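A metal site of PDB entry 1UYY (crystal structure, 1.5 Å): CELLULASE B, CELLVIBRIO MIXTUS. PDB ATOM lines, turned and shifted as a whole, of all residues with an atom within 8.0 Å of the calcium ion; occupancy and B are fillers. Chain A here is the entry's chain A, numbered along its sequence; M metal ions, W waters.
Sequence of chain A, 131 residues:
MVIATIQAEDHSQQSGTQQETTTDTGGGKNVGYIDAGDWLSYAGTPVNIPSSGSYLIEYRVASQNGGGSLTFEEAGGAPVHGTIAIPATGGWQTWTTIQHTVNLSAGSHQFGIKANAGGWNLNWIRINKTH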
ATOM      1  N   ILE A   6      -1.685  -9.044 -24.914  1.00  0.00           N
ATOM      2  CA  ILE A   6      -2.311  -8.379 -26.053  1.00  0.00           C
ATOM      3  C   ILE A   6      -2.353  -6.901 -25.762  1.00  0.00           C
ATOM      4  O   ILE A   6      -2.976  -6.478 -24.798  1.00  0.00           O
ATOM      5  CB  ILE A   6      -3.734  -8.929 -26.248  1.00  0.00           C
ATOM      6  CG1 ILE A   6      -3.690 -10.413 -26.665  1.00  0.00           C
ATOM      7  CG2 ILE A   6      -4.507  -8.112 -27.274  1.00  0.00           C
ATOM      8  CD1 ILE A   6      -5.021 -11.114 -26.543  1.00  0.00           C
ATOM      9  N   GLN A   7      -1.669  -6.100 -26.571  1.00  0.00           N
ATOM     10  CA  GLN A   7      -1.806  -4.650 -26.467  1.00  0.00           C
ATOM     11  C   GLN A   7      -3.225  -4.282 -26.894  1.00  0.00           C
ATOM     12  O   GLN A   7      -3.735  -4.774 -27.903  1.00  0.00           O
ATOM     13  CB  GLN A   7      -0.764  -3.939 -27.324  1.00  0.00           C
ATOM     14  CG  GLN A   7       0.663  -4.185 -26.864  1.00  0.00           C
ATOM     15  CD  GLN A   7       0.930  -3.611 -25.476  1.00  0.00           C
ATOM     16  OE1 GLN A   7       0.436  -2.523 -25.132  1.00  0.00           O
ATOM     17  NE2 GLN A   7       1.699  -4.337 -24.663  1.00  0.00           N
ATOM     18  N   ALA A   8      -3.874  -3.429 -26.105  1.00  0.00           N
ATOM     19  CA  ALA A   8      -5.298  -3.161 -26.300  1.00  0.00           C
ATOM     20  C   ALA A   8      -5.618  -2.544 -27.649  1.00  0.00           C
ATOM     21  O   ALA A   8      -6.684  -2.769 -28.216  1.00  0.00           O
ATOM     22  CB  ALA A   8      -5.832  -2.278 -25.200  1.00  0.00           C
ATOM     23  N   GLU A   9      -4.673  -1.755 -28.157  1.00  0.00           N
ATOM     24  CA  GLU A   9      -4.816  -1.105 -29.447  1.00  0.00           C
ATOM     25  C   GLU A   9      -4.675  -2.064 -30.634  1.00  0.00           C
ATOM     26  O   GLU A   9      -5.057  -1.714 -31.749  1.00  0.00           O
ATOM     27  CB  GLU A   9      -3.810   0.054 -29.571  1.00  0.00           C
ATOM     28  CG  GLU A   9      -2.329  -0.339 -29.714  1.00  0.00           C
ATOM     29  CD  GLU A   9      -1.583  -0.546 -28.400  1.00  0.00           C
ATOM     30  OE1 GLU A   9      -2.197  -0.713 -27.324  1.00  0.00           O
ATOM     31  OE2 GLU A   9      -0.324  -0.555 -28.446  1.00  0.00           O
ATOM     32  N   ASP A  10      -4.150  -3.275 -30.400  1.00  0.00           N
ATOM     33  CA  ASP A  10      -3.948  -4.272 -31.467  1.00  0.00           C
ATOM     34  C   ASP A  10      -5.187  -5.142 -31.717  1.00  0.00           C
ATOM     35  O   ASP A  10      -5.115  -6.361 -31.869  1.00  0.00           O
ATOM     36  CB  ASP A  10      -2.737  -5.154 -31.141  1.00  0.00           C
ATOM     37  CG  ASP A  10      -1.417  -4.412 -31.231  1.00  0.00           C
ATOM     38  OD1 ASP A  10      -1.378  -3.280 -31.763  1.00  0.00           O
ATOM     39  OD2 ASP A  10      -0.377  -4.912 -30.792  1.00  0.00           O
ATOM     40  N   GLN A  19      -7.482   5.354 -30.257  1.00  0.00           N
ATOM     41  CA  GLN A  19      -6.125   5.206 -29.756  1.00  0.00           C
ATOM     42  C   GLN A  19      -5.562   6.559 -29.332  1.00  0.00           C
ATOM     43  O   GLN A  19      -5.922   7.597 -29.892  1.00  0.00           O
ATOM     44  CB  GLN A  19      -5.284   4.637 -30.898  1.00  0.00           C
ATOM     45  CG  GLN A  19      -3.846   4.394 -30.625  1.00  0.00           C
ATOM     46  CD  GLN A  19      -3.176   3.809 -31.842  1.00  0.00           C
ATOM     47  OE1 GLN A  19      -3.319   2.619 -32.117  1.00  0.00           O
ATOM     48  NE2 GLN A  19      -2.474   4.653 -32.599  1.00  0.00           N
ATOM     49  N   GLU A  20      -4.679   6.536 -28.341  1.00  0.00           N
ATOM     50  CA  GLU A  20      -3.933   7.721 -27.942  1.00  0.00           C
ATOM     51  C   GLU A  20      -2.604   7.303 -27.314  1.00  0.00           C
ATOM     52  O   GLU A  20      -2.442   6.157 -26.914  1.00  0.00           O
ATOM     53  CB  GLU A  20      -4.757   8.565 -26.957  1.00  0.00           C
ATOM     54  CG  GLU A  20      -5.095   7.853 -25.661  1.00  0.00           C
ATOM     55  CD  GLU A  20      -6.103   8.578 -24.777  1.00  0.00           C
ATOM     56  OE1 GLU A  20      -6.578   9.688 -25.135  1.00  0.00           O
ATOM     57  OE2 GLU A  20      -6.424   8.032 -23.708  1.00  0.00           O
ATOM     58  N   THR A  22       0.244   6.714 -24.658  1.00  0.00           N
ATOM     59  CA  THR A  22       0.305   6.503 -23.215  1.00  0.00           C
ATOM     60  C   THR A  22       1.684   6.831 -22.662  1.00  0.00           C
ATOM     61  O   THR A  22       2.693   6.619 -23.337  1.00  0.00           O
ATOM     62  CB  THR A  22      -0.099   5.046 -22.848  1.00  0.00           C
ATOM     63  OG1 THR A  22      -0.133   4.913 -21.430  1.00  0.00           O
ATOM     64  CG2 THR A  22       0.952   4.009 -23.309  1.00  0.00           C
ATOM     65  N   ASP A  24       2.440   5.367 -19.722  1.00  0.00           N
ATOM     66  CA  ASP A  24       2.715   4.181 -18.915  1.00  0.00           C
ATOM     67  C   ASP A  24       4.083   3.606 -19.285  1.00  0.00           C
ATOM     68  O   ASP A  24       4.611   3.897 -20.354  1.00  0.00           O
ATOM     69  CB  ASP A  24       1.618   3.136 -19.169  1.00  0.00           C
ATOM     70  CG  ASP A  24       1.595   2.045 -18.120  1.00  0.00           C
ATOM     71  OD1 ASP A  24       2.188   2.203 -17.030  1.00  0.00           O
ATOM     72  OD2 ASP A  24       0.996   0.962 -18.315  1.00  0.00           O
ATOM     73  N   THR A  25       4.644   2.807 -18.385  1.00  0.00           N
ATOM     74  CA  THR A  25       5.876   2.047 -18.619  1.00  0.00           C
ATOM     75  C   THR A  25       5.861   1.354 -19.984  1.00  0.00           C
ATOM     76  O   THR A  25       4.892   0.667 -20.307  1.00  0.00           O
ATOM     77  CB  THR A  25       6.046   0.973 -17.516  1.00  0.00           C
ATOM     78  OG1 THR A  25       5.871   1.569 -16.226  1.00  0.00           O
ATOM     79  CG2 THR A  25       7.459   0.413 -17.481  1.00  0.00           C
ATOM     80  N   GLY A  26       6.924   1.541 -20.763  1.00  0.00           N
ATOM     81  CA  GLY A  26       7.021   0.967 -22.094  1.00  0.00           C
ATOM     82  C   GLY A  26       6.469   1.849 -23.201  1.00  0.00           C
ATOM     83  O   GLY A  26       6.706   1.582 -24.377  1.00  0.00           O
ATOM     84  N   GLY A  27       5.744   2.907 -22.830  1.00  0.00           N
ATOM     85  CA  GLY A  27       5.170   3.829 -23.800  1.00  0.00           C
ATOM     86  C   GLY A  27       4.170   3.155 -24.730  1.00  0.00           C
ATOM     87  O   GLY A  27       3.491   2.200 -24.357  1.00  0.00           O
ATOM     88  N   GLY A  28       4.112   3.651 -25.963  1.00  0.00           N
ATOM     89  CA  GLY A  28       3.207   3.121 -26.965  1.00  0.00           C
ATOM     90  C   GLY A  28       1.852   3.803 -26.919  1.00  0.00           C
ATOM     91  O   GLY A  28       1.767   5.033 -26.784  1.00  0.00           O
ATOM     92  N   LYS A  29       0.787   3.013 -27.015  1.00  0.00           N
ATOM     93  CA  LYS A  29      -0.565   3.538 -27.095  1.00  0.00           C
ATOM     94  C   LYS A  29      -1.504   2.864 -26.110  1.00  0.00           C
ATOM     95  O   LYS A  29      -1.272   1.733 -25.690  1.00  0.00           O
ATOM     96  CB  LYS A  29      -1.140   3.324 -28.502  1.00  0.00           C
ATOM     97  CG  LYS A  29      -0.263   3.851 -29.635  1.00  0.00           C
ATOM     98  CD  LYS A  29      -0.268   5.354 -29.660  1.00  0.00           C
ATOM     99  CE  LYS A  29       0.553   5.894 -30.818  1.00  0.00           C
ATOM    100  NZ  LYS A  29       0.422   7.366 -30.936  1.00  0.00           N
ATOM    101  N   ASN A  30      -2.555   3.571 -25.737  1.00  0.00           N
ATOM    102  CA  ASN A  30      -3.694   2.949 -25.057  1.00  0.00           C
ATOM    103  C   ASN A  30      -4.976   3.242 -25.804  1.00  0.00           C
ATOM    104  O   ASN A  30      -5.036   4.141 -26.640  1.00  0.00           O
ATOM    105  CB  ASN A  30      -3.797   3.395 -23.584  1.00  0.00           C
ATOM    106  CG  ASN A  30      -4.234   4.840 -23.419  1.00  0.00           C
ATOM    107  OD1 ASN A  30      -5.435   5.163 -23.397  1.00  0.00           O
ATOM    108  ND2 ASN A  30      -3.264   5.713 -23.254  1.00  0.00           N
ATOM    109  N   VAL A  31      -6.006   2.465 -25.494  1.00  0.00           N
ATOM    110  CA  VAL A  31      -7.346   2.733 -25.985  1.00  0.00           C
ATOM    111  C   VAL A  31      -8.018   3.704 -25.028  1.00  0.00           C
ATOM    112  O   VAL A  31      -7.952   3.518 -23.817  1.00  0.00           O
ATOM    113  CB  VAL A  31      -8.159   1.451 -26.073  1.00  0.00           C
ATOM    114  CG1 VAL A  31      -9.620   1.742 -26.497  1.00  0.00           C
ATOM    115  CG2 VAL A  31      -7.520   0.487 -27.046  1.00  0.00           C
ATOM    116  N   ARG A  60      -4.426  -3.680 -17.746  1.00  0.00           N
ATOM    117  CA  ARG A  60      -3.661  -2.489 -17.389  1.00  0.00           C
ATOM    118  C   ARG A  60      -4.554  -1.296 -17.695  1.00  0.00           C
ATOM    119  O   ARG A  60      -4.808  -0.995 -18.853  1.00  0.00           O
ATOM    120  CB  ARG A  60      -2.358  -2.453 -18.194  1.00  0.00           C
ATOM    121  CG  ARG A  60      -1.375  -1.374 -17.757  1.00  0.00           C
ATOM    122  CD  ARG A  60      -0.838  -1.578 -16.354  1.00  0.00           C
ATOM    123  NE  ARG A  60       0.210  -0.617 -16.046  1.00  0.00           N
ATOM    124  CZ  ARG A  60       0.805  -0.508 -14.855  1.00  0.00           C
ATOM    125  NH1 ARG A  60       0.460  -1.301 -13.850  1.00  0.00           N
ATOM    126  NH2 ARG A  60       1.741   0.411 -14.696  1.00  0.00           N
ATOM    127  N   TRP A  95      -1.621   4.500 -13.962  1.00  0.00           N
ATOM    128  CA  TRP A  95      -1.887   3.123 -14.382  1.00  0.00           C
ATOM    129  C   TRP A  95      -1.764   2.103 -13.251  1.00  0.00           C
ATOM    130  O   TRP A  95      -0.892   2.199 -12.383  1.00  0.00           O
ATOM    131  CB  TRP A  95      -0.933   2.744 -15.512  1.00  0.00           C
ATOM    132  CG  TRP A  95      -1.197   3.565 -16.727  1.00  0.00           C
ATOM    133  CD1 TRP A  95      -0.584   4.723 -17.084  1.00  0.00           C
ATOM    134  CD2 TRP A  95      -2.198   3.308 -17.723  1.00  0.00           C
ATOM    135  NE1 TRP A  95      -1.127   5.202 -18.247  1.00  0.00           N
ATOM    136  CE2 TRP A  95      -2.124   4.361 -18.661  1.00  0.00           C
ATOM    137  CE3 TRP A  95      -3.150   2.297 -17.916  1.00  0.00           C
ATOM    138  CZ2 TRP A  95      -2.955   4.423 -19.780  1.00  0.00           C
ATOM    139  CZ3 TRP A  95      -3.971   2.360 -19.025  1.00  0.00           C
ATOM    140  CH2 TRP A  95      -3.876   3.413 -19.944  1.00  0.00           C
ATOM    141  N   LEU A 122      -7.434   1.690 -21.424  1.00  0.00           N
ATOM    142  CA  LEU A 122      -6.888   0.331 -21.407  1.00  0.00           C
ATOM    143  C   LEU A 122      -5.599   0.270 -22.227  1.00  0.00           C
ATOM    144  O   LEU A 122      -5.603   0.607 -23.413  1.00  0.00           O
ATOM    145  CB  LEU A 122      -7.917  -0.653 -21.961  1.00  0.00           C
ATOM    146  CG  LEU A 122      -7.572  -2.146 -21.935  1.00  0.00           C
ATOM    147  CD1 LEU A 122      -7.440  -2.684 -20.521  1.00  0.00           C
ATOM    148  CD2 LEU A 122      -8.607  -2.957 -22.723  1.00  0.00           C
ATOM    149  N   ASN A 123      -4.504  -0.168 -21.609  1.00  0.00           N
ATOM    150  CA  ASN A 123      -3.191  -0.278 -22.267  1.00  0.00           C
ATOM    151  C   ASN A 123      -2.968  -1.655 -22.886  1.00  0.00           C
ATOM    152  O   ASN A 123      -2.597  -1.768 -24.051  1.00  0.00           O
ATOM    153  CB  ASN A 123      -2.081   0.072 -21.265  1.00  0.00           C
ATOM    154  CG  ASN A 123      -0.727   0.260 -21.909  1.00  0.00           C
ATOM    155  OD1 ASN A 123      -0.577   0.159 -23.107  1.00  0.00           O
ATOM    156  ND2 ASN A 123       0.287   0.515 -21.081  1.00  0.00           N
ATOM    157  N   TRP A 124      -3.169  -2.695 -22.081  1.00  0.00           N
ATOM    158  CA  TRP A 124      -2.976  -4.080 -22.513  1.00  0.00           C
ATOM    159  C   TRP A 124      -3.752  -5.039 -21.616  1.00  0.00           C
ATOM    160  O   TRP A 124      -4.241  -4.651 -20.546  1.00  0.00           O
ATOM    161  CB  TRP A 124      -1.479  -4.457 -22.581  1.00  0.00           C
ATOM    162  CG  TRP A 124      -0.644  -4.128 -21.358  1.00  0.00           C
ATOM    163  CD1 TRP A 124       0.239  -3.092 -21.247  1.00  0.00           C
ATOM    164  CD2 TRP A 124      -0.562  -4.855 -20.126  1.00  0.00           C
ATOM    165  NE1 TRP A 124       0.840  -3.114 -20.008  1.00  0.00           N
ATOM    166  CE2 TRP A 124       0.375  -4.178 -19.305  1.00  0.00           C
ATOM    167  CE3 TRP A 124      -1.191  -5.995 -19.618  1.00  0.00           C
ATOM    168  CZ2 TRP A 124       0.686  -4.610 -18.010  1.00  0.00           C
ATOM    169  CZ3 TRP A 124      -0.881  -6.424 -18.333  1.00  0.00           C
ATOM    170  CH2 TRP A 124       0.042  -5.733 -17.538  1.00  0.00           C
ATOM    171  N   ILE A 125      -3.848  -6.279 -22.084  1.00  0.00           N
ATOM    172  CA  ILE A 125      -4.484  -7.398 -21.394  1.00  0.00           C
ATOM    173  C   ILE A 125      -3.470  -8.536 -21.350  1.00  0.00           C
ATOM    174  O   ILE A 125      -2.667  -8.673 -22.271  1.00  0.00           O
ATOM    175  CB  ILE A 125      -5.740  -7.866 -22.168  1.00  0.00           C
ATOM    176  CG1 ILE A 125      -6.698  -6.699 -22.447  1.00  0.00           C
ATOM    177  CG2 ILE A 125      -6.458  -8.988 -21.432  1.00  0.00           C
ATOM    178  CD1 ILE A 125      -6.813  -6.407 -23.927  1.00  0.00           C
HETATM  179 CA    CA M   1      -0.783  -0.503 -25.301  1.00  0.00          CA
HETATM  180  O   HOH W   1       1.472   0.135 -25.990  1.00  0.00           O
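O of Asn 123 lies close to N of Ala 8, at 2.9 Å.
OD2 of Asp 24 is in hydrogen-bond range of ND2 of Asn 123.
O of Arg 60 is in hydrogen-bond range of N of Asn 123 (2.9 Å).
The nearest printed residue that does not touch the calcium ion is Ala 8 (4.3 Å).
The calcium ion is bound by OD1 of Asn 123 (2.3 Å), O of Lys 29 (2.3 Å), OE1 of Gln 7 (2.4 Å), water W1 (2.4 Å), OE1 of Glu 9 (2.5 Å) and O of Asn 123 (2.5 Å).
Water W1 lies within hydrogen-bond range of the side-chain carboxylate (OE2) of Glu 9 (3.1 Å), the backbone NH (N) of Lys 29 (3.1 Å) and the backbone carbonyl oxygen (O) of Gly 27 (3.3 Å).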
